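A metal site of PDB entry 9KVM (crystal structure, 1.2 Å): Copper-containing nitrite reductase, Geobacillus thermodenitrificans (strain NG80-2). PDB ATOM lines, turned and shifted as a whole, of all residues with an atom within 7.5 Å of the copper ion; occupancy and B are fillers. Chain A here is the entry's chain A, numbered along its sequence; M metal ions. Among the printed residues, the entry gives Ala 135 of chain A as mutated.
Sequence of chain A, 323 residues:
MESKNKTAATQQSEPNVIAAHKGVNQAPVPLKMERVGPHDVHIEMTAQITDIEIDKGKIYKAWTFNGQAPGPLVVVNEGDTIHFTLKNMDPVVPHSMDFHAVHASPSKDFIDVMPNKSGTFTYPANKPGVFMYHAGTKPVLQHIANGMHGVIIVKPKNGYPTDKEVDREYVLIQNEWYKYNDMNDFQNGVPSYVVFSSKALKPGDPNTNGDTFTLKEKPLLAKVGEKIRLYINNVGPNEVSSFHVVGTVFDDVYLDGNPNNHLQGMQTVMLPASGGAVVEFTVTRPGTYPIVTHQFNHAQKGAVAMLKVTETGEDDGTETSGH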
ATOM      1  N   ALA A  47     -15.937   1.834 -16.552  1.00  0.00           N
ATOM      2  CA  ALA A  47     -14.484   1.772 -16.586  1.00  0.00           C
ATOM      3  C   ALA A  47     -14.040   2.675 -17.722  1.00  0.00           C
ATOM      4  O   ALA A  47     -14.547   2.534 -18.849  1.00  0.00           O
ATOM      5  CB  ALA A  47     -13.995   0.347 -16.820  1.00  0.00           C
ATOM      6  N   ILE A  49     -10.864   5.798 -19.206  1.00  0.00           N
ATOM      7  CA  ILE A  49      -9.488   6.290 -19.198  1.00  0.00           C
ATOM      8  C   ILE A  49      -9.555   7.802 -19.131  1.00  0.00           C
ATOM      9  O   ILE A  49     -10.099   8.437 -20.033  1.00  0.00           O
ATOM     10  CB  ILE A  49      -8.775   5.814 -20.479  1.00  0.00           C
ATOM     11  CG1 ILE A  49      -8.824   4.284 -20.613  1.00  0.00           C
ATOM     12  CG2 ILE A  49      -7.363   6.356 -20.524  1.00  0.00           C
ATOM     13  CD1 ILE A  49      -8.316   3.504 -19.402  1.00  0.00           C
ATOM     14  N   TRP A  63      -6.480   4.631 -15.237  1.00  0.00           N
ATOM     15  CA  TRP A  63      -7.512   3.644 -15.462  1.00  0.00           C
ATOM     16  C   TRP A  63      -8.483   3.792 -14.312  1.00  0.00           C
ATOM     17  O   TRP A  63      -8.111   3.571 -13.166  1.00  0.00           O
ATOM     18  CB  TRP A  63      -6.913   2.238 -15.458  1.00  0.00           C
ATOM     19  CG  TRP A  63      -5.901   1.960 -16.508  1.00  0.00           C
ATOM     20  CD1 TRP A  63      -5.325   2.833 -17.365  1.00  0.00           C
ATOM     21  CD2 TRP A  63      -5.335   0.673 -16.775  1.00  0.00           C
ATOM     22  NE1 TRP A  63      -4.422   2.166 -18.170  1.00  0.00           N
ATOM     23  CE2 TRP A  63      -4.412   0.837 -17.824  1.00  0.00           C
ATOM     24  CE3 TRP A  63      -5.492  -0.576 -16.203  1.00  0.00           C
ATOM     25  CZ2 TRP A  63      -3.674  -0.242 -18.344  1.00  0.00           C
ATOM     26  CZ3 TRP A  63      -4.773  -1.639 -16.694  1.00  0.00           C
ATOM     27  CH2 TRP A  63      -3.871  -1.469 -17.765  1.00  0.00           C
ATOM     28  N   THR A  64      -9.712   4.198 -14.607  1.00  0.00           N
ATOM     29  CA  THR A  64     -10.612   4.639 -13.545  1.00  0.00           C
ATOM     30  C   THR A  64     -11.966   3.961 -13.620  1.00  0.00           C
ATOM     31  O   THR A  64     -12.406   3.482 -14.671  1.00  0.00           O
ATOM     32  CB  THR A  64     -10.878   6.159 -13.583  1.00  0.00           C
ATOM     33  OG1 THR A  64     -11.709   6.487 -14.700  1.00  0.00           O
ATOM     34  CG2 THR A  64      -9.584   6.955 -13.645  1.00  0.00           C
ATOM     35  N   PHE A  65     -12.671   4.038 -12.487  1.00  0.00           N
ATOM     36  CA  PHE A  65     -14.119   3.929 -12.477  1.00  0.00           C
ATOM     37  C   PHE A  65     -14.703   5.340 -12.522  1.00  0.00           C
ATOM     38  O   PHE A  65     -14.400   6.168 -11.647  1.00  0.00           O
ATOM     39  CB  PHE A  65     -14.553   3.215 -11.210  1.00  0.00           C
ATOM     40  CG  PHE A  65     -14.062   1.796 -11.132  1.00  0.00           C
ATOM     41  CD1 PHE A  65     -14.584   0.822 -11.965  1.00  0.00           C
ATOM     42  CD2 PHE A  65     -13.103   1.441 -10.211  1.00  0.00           C
ATOM     43  CE1 PHE A  65     -14.149  -0.496 -11.876  1.00  0.00           C
ATOM     44  CE2 PHE A  65     -12.661   0.123 -10.101  1.00  0.00           C
ATOM     45  CZ  PHE A  65     -13.183  -0.850 -10.948  1.00  0.00           C
ATOM     46  N   ASN A  88     -17.813  -0.977 -19.761  1.00  0.00           N
ATOM     47  CA  ASN A  88     -16.391  -0.777 -20.072  1.00  0.00           C
ATOM     48  C   ASN A  88     -16.237   0.117 -21.294  1.00  0.00           C
ATOM     49  O   ASN A  88     -16.551  -0.293 -22.416  1.00  0.00           O
ATOM     50  CB  ASN A  88     -15.710  -2.115 -20.303  1.00  0.00           C
ATOM     51  CG  ASN A  88     -14.213  -1.970 -20.431  1.00  0.00           C
ATOM     52  OD1 ASN A  88     -13.696  -0.859 -20.349  1.00  0.00           O
ATOM     53  ND2 ASN A  88     -13.512  -3.072 -20.628  1.00  0.00           N
ATOM     54  N   ASP A  90     -13.237   1.510 -22.021  1.00  0.00           N
ATOM     55  CA  ASP A  90     -11.868   1.402 -22.492  1.00  0.00           C
ATOM     56  C   ASP A  90     -11.870   0.767 -23.872  1.00  0.00           C
ATOM     57  O   ASP A  90     -12.527  -0.274 -24.054  1.00  0.00           O
ATOM     58  CB  ASP A  90     -11.110   0.528 -21.498  1.00  0.00           C
ATOM     59  CG  ASP A  90      -9.608   0.475 -21.743  1.00  0.00           C
ATOM     60  OD1 ASP A  90      -9.143   0.374 -22.897  1.00  0.00           O
ATOM     61  OD2 ASP A  90      -8.883   0.469 -20.731  1.00  0.00           O
ATOM     62  N   VAL A  93      -8.628  -2.582 -23.157  1.00  0.00           N
ATOM     63  CA  VAL A  93      -8.314  -3.357 -21.958  1.00  0.00           C
ATOM     64  C   VAL A  93      -9.607  -3.816 -21.282  1.00  0.00           C
ATOM     65  O   VAL A  93     -10.470  -2.982 -21.013  1.00  0.00           O
ATOM     66  CB  VAL A  93      -7.418  -2.566 -20.969  1.00  0.00           C
ATOM     67  CG1 VAL A  93      -7.042  -3.440 -19.788  1.00  0.00           C
ATOM     68  CG2 VAL A  93      -6.167  -2.033 -21.656  1.00  0.00           C
ATOM     69  N   PRO A  94      -9.748  -5.101 -20.953  1.00  0.00           N
ATOM     70  CA  PRO A  94     -10.868  -5.526 -20.100  1.00  0.00           C
ATOM     71  C   PRO A  94     -10.717  -4.997 -18.693  1.00  0.00           C
ATOM     72  O   PRO A  94      -9.608  -4.793 -18.197  1.00  0.00           O
ATOM     73  CB  PRO A  94     -10.764  -7.054 -20.117  1.00  0.00           C
ATOM     74  CG  PRO A  94      -9.748  -7.395 -21.120  1.00  0.00           C
ATOM     75  CD  PRO A  94      -8.852  -6.221 -21.272  1.00  0.00           C
ATOM     76  N   HIS A  95     -11.863  -4.817 -18.013  1.00  0.00           N
ATOM     77  CA  HIS A  95     -11.865  -4.429 -16.611  1.00  0.00           C
ATOM     78  C   HIS A  95     -12.966  -5.200 -15.897  1.00  0.00           C
ATOM     79  O   HIS A  95     -13.821  -5.818 -16.521  1.00  0.00           O
ATOM     80  CB  HIS A  95     -12.026  -2.911 -16.391  1.00  0.00           C
ATOM     81  CG  HIS A  95     -10.995  -2.111 -17.126  1.00  0.00           C
ATOM     82  ND1 HIS A  95      -9.714  -1.935 -16.663  1.00  0.00           N
ATOM     83  CD2 HIS A  95     -11.066  -1.445 -18.303  1.00  0.00           C
ATOM     84  CE1 HIS A  95      -9.039  -1.206 -17.525  1.00  0.00           C
ATOM     85  NE2 HIS A  95      -9.846  -0.880 -18.529  1.00  0.00           N
ATOM     86  N   SER A  96     -12.944  -5.159 -14.584  1.00  0.00           N
ATOM     87  CA  SER A  96     -13.881  -5.905 -13.751  1.00  0.00           C
ATOM     88  C   SER A  96     -14.015  -5.181 -12.418  1.00  0.00           C
ATOM     89  O   SER A  96     -13.304  -4.215 -12.155  1.00  0.00           O
ATOM     90  CB  SER A  96     -13.377  -7.322 -13.467  1.00  0.00           C
ATOM     91  OG  SER A  96     -12.147  -7.298 -12.787  1.00  0.00           O
ATOM     92  N   HIS A 134     -12.045  -2.658  -6.105  1.00  0.00           N
ATOM     93  CA  HIS A 134     -10.992  -2.504  -7.095  1.00  0.00           C
ATOM     94  C   HIS A 134     -11.254  -3.454  -8.252  1.00  0.00           C
ATOM     95  O   HIS A 134     -12.053  -4.373  -8.140  1.00  0.00           O
ATOM     96  CB  HIS A 134      -9.586  -2.760  -6.475  1.00  0.00           C
ATOM     97  CG  HIS A 134      -9.414  -4.122  -5.878  1.00  0.00           C
ATOM     98  ND1 HIS A 134      -9.100  -5.239  -6.618  1.00  0.00           N
ATOM     99  CD2 HIS A 134      -9.501  -4.538  -4.586  1.00  0.00           C
ATOM    100  CE1 HIS A 134      -9.014  -6.291  -5.816  1.00  0.00           C
ATOM    101  NE2 HIS A 134      -9.251  -5.887  -4.582  1.00  0.00           N
ATOM    102  N   ALA A 135     -10.532  -3.244  -9.340  1.00  0.00           N
ATOM    103  CA  ALA A 135     -10.608  -4.161 -10.455  1.00  0.00           C
ATOM    104  C   ALA A 135      -9.958  -5.493 -10.084  1.00  0.00           C
ATOM    105  O   ALA A 135      -9.005  -5.547  -9.317  1.00  0.00           O
ATOM    106  CB  ALA A 135      -9.918  -3.594 -11.694  1.00  0.00           C
ATOM    107  N   GLY A 136     -10.515  -6.569 -10.626  1.00  0.00           N
ATOM    108  CA  GLY A 136     -10.050  -7.920 -10.382  1.00  0.00           C
ATOM    109  C   GLY A 136      -9.377  -8.550 -11.581  1.00  0.00           C
ATOM    110  O   GLY A 136      -9.132  -9.758 -11.562  1.00  0.00           O
ATOM    111  N   THR A 137      -9.050  -7.776 -12.606  1.00  0.00           N
ATOM    112  CA  THR A 137      -8.512  -8.286 -13.859  1.00  0.00           C
ATOM    113  C   THR A 137      -7.006  -8.479 -13.722  1.00  0.00           C
ATOM    114  O   THR A 137      -6.299  -7.630 -13.181  1.00  0.00           O
ATOM    115  CB  THR A 137      -8.803  -7.238 -14.936  1.00  0.00           C
ATOM    116  OG1 THR A 137     -10.216  -7.021 -14.985  1.00  0.00           O
ATOM    117  CG2 THR A 137      -8.328  -7.651 -16.320  1.00  0.00           C
ATOM    118  N   PRO A 139      -3.142  -8.471 -14.705  1.00  0.00           N
ATOM    119  CA  PRO A 139      -2.574  -8.513 -13.338  1.00  0.00           C
ATOM    120  C   PRO A 139      -3.252  -7.482 -12.458  1.00  0.00           C
ATOM    121  O   PRO A 139      -3.294  -6.290 -12.812  1.00  0.00           O
ATOM    122  CB  PRO A 139      -1.093  -8.154 -13.547  1.00  0.00           C
ATOM    123  CG  PRO A 139      -0.909  -7.956 -15.011  1.00  0.00           C
ATOM    124  CD  PRO A 139      -2.244  -7.768 -15.633  1.00  0.00           C
ATOM    125  N   VAL A 140      -3.782  -7.922 -11.328  1.00  0.00           N
ATOM    126  CA  VAL A 140      -4.530  -7.016 -10.449  1.00  0.00           C
ATOM    127  C   VAL A 140      -3.666  -5.825 -10.027  1.00  0.00           C
ATOM    128  O   VAL A 140      -4.136  -4.693  -9.992  1.00  0.00           O
ATOM    129  CB  VAL A 140      -5.115  -7.795  -9.254  1.00  0.00           C
ATOM    130  CG1 VAL A 140      -5.788  -6.850  -8.257  1.00  0.00           C
ATOM    131  CG2 VAL A 140      -6.090  -8.840  -9.741  1.00  0.00           C
ATOM    132  N   GLN A 142      -1.516  -4.201 -11.664  1.00  0.00           N
ATOM    133  CA  GLN A 142      -1.500  -3.179 -12.706  1.00  0.00           C
ATOM    134  C   GLN A 142      -2.765  -2.336 -12.709  1.00  0.00           C
ATOM    135  O   GLN A 142      -2.705  -1.116 -12.846  1.00  0.00           O
ATOM    136  CB  GLN A 142      -1.324  -3.853 -14.069  1.00  0.00           C
ATOM    137  CG  GLN A 142      -1.132  -2.875 -15.187  1.00  0.00           C
ATOM    138  CD  GLN A 142      -0.833  -3.559 -16.498  1.00  0.00           C
ATOM    139  OE1 GLN A 142      -1.093  -4.762 -16.656  1.00  0.00           O
ATOM    140  NE2 GLN A 142      -0.318  -2.804 -17.463  1.00  0.00           N
ATOM    141  N   HIS A 143      -3.926  -2.979 -12.543  1.00  0.00           N
ATOM    142  CA  HIS A 143      -5.180  -2.238 -12.516  1.00  0.00           C
ATOM    143  C   HIS A 143      -5.282  -1.361 -11.273  1.00  0.00           C
ATOM    144  O   HIS A 143      -5.708  -0.202 -11.392  1.00  0.00           O
ATOM    145  CB  HIS A 143      -6.367  -3.189 -12.615  1.00  0.00           C
ATOM    146  CG  HIS A 143      -6.484  -3.796 -13.962  1.00  0.00           C
ATOM    147  ND1 HIS A 143      -7.437  -3.400 -14.866  1.00  0.00           N
ATOM    148  CD2 HIS A 143      -5.745  -4.748 -14.567  1.00  0.00           C
ATOM    149  CE1 HIS A 143      -7.294  -4.103 -15.977  1.00  0.00           C
ATOM    150  NE2 HIS A 143      -6.269  -4.927 -15.824  1.00  0.00           N
ATOM    151  N   ILE A 144      -4.894  -1.865 -10.107  1.00  0.00           N
ATOM    152  CA  ILE A 144      -4.965  -1.031  -8.902  1.00  0.00           C
ATOM    153  C   ILE A 144      -4.005   0.142  -9.017  1.00  0.00           C
ATOM    154  O   ILE A 144      -4.385   1.292  -8.780  1.00  0.00           O
ATOM    155  CB  ILE A 144      -4.707  -1.830  -7.620  1.00  0.00           C
ATOM    156  CG1 ILE A 144      -5.777  -2.927  -7.427  1.00  0.00           C
ATOM    157  CG2 ILE A 144      -4.721  -0.873  -6.428  1.00  0.00           C
ATOM    158  CD1 ILE A 144      -5.475  -3.865  -6.251  1.00  0.00           C
ATOM    159  N   ASN A 146      -2.803   1.662 -11.514  1.00  0.00           N
ATOM    160  CA  ASN A 146      -3.177   2.640 -12.520  1.00  0.00           C
ATOM    161  C   ASN A 146      -4.437   3.425 -12.151  1.00  0.00           C
ATOM    162  O   ASN A 146      -4.802   4.340 -12.883  1.00  0.00           O
ATOM    163  CB  ASN A 146      -3.352   2.003 -13.891  1.00  0.00           C
ATOM    164  CG  ASN A 146      -2.025   1.746 -14.605  1.00  0.00           C
ATOM    165  OD1 ASN A 146      -1.045   2.482 -14.439  1.00  0.00           O
ATOM    166  ND2 ASN A 146      -2.006   0.720 -15.412  1.00  0.00           N
ATOM    167  N   GLY A 147      -5.080   3.126 -11.016  1.00  0.00           N
ATOM    168  CA  GLY A 147      -6.153   3.959 -10.511  1.00  0.00           C
ATOM    169  C   GLY A 147      -7.474   3.259 -10.204  1.00  0.00           C
ATOM    170  O   GLY A 147      -8.407   3.928  -9.754  1.00  0.00           O
ATOM    171  N   MET A 148      -7.575   1.946 -10.413  1.00  0.00           N
ATOM    172  CA  MET A 148      -8.881   1.278 -10.287  1.00  0.00           C
ATOM    173  C   MET A 148      -9.099   0.770  -8.876  1.00  0.00           C
ATOM    174  O   MET A 148      -9.003  -0.428  -8.584  1.00  0.00           O
ATOM    175  CB  MET A 148      -9.036   0.148 -11.302  1.00  0.00           C
ATOM    176  CG  MET A 148      -9.263   0.642 -12.670  1.00  0.00           C
ATOM    177  SD  MET A 148     -10.095  -0.593 -13.717  1.00  0.00           S
ATOM    178  CE  MET A 148     -10.882   0.537 -14.839  1.00  0.00           C
HETATM  179 CU    CU M   1      -8.899  -2.060 -14.749  1.00  0.00          CU
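A ring nitrogen (NE2) of His 95 lies close to the backbone carbonyl oxygen (O) of Val 93, 3.3 Å away.
A ring nitrogen (NE2) of His 95 is in hydrogen-bond range of the side-chain carboxylate of Asp 90 (2.8 Å).
The backbone NH of Ala 135 sits at hydrogen-bond distance from the backbone carbonyl oxygen of Met 148 (3.3 Å).
The backbone NH (N) of Met 148 lies close to the backbone carbonyl oxygen (O) of Trp 63 (3.2 Å).
The backbone NH (N) of Trp 63 lies within hydrogen-bond range of the backbone carbonyl oxygen (O) of Asn 146, 2.9 Å away.
Merely in contact with the copper ion: Ala 135 and Trp 63.
Within 4 Å of the copper ion: Trp 63, His 95, Ala 135, His 143 and Met 148.
The nearest printed residue that does not touch the copper ion is Pro 94 (4.5 Å).
The copper ion is bound by a ring nitrogen (ND1) of His 143 (2.0 Å), a ring nitrogen (ND1) of His 95 (2.1 Å) and the side-chain sulfur of Met 148 (2.2 Å).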
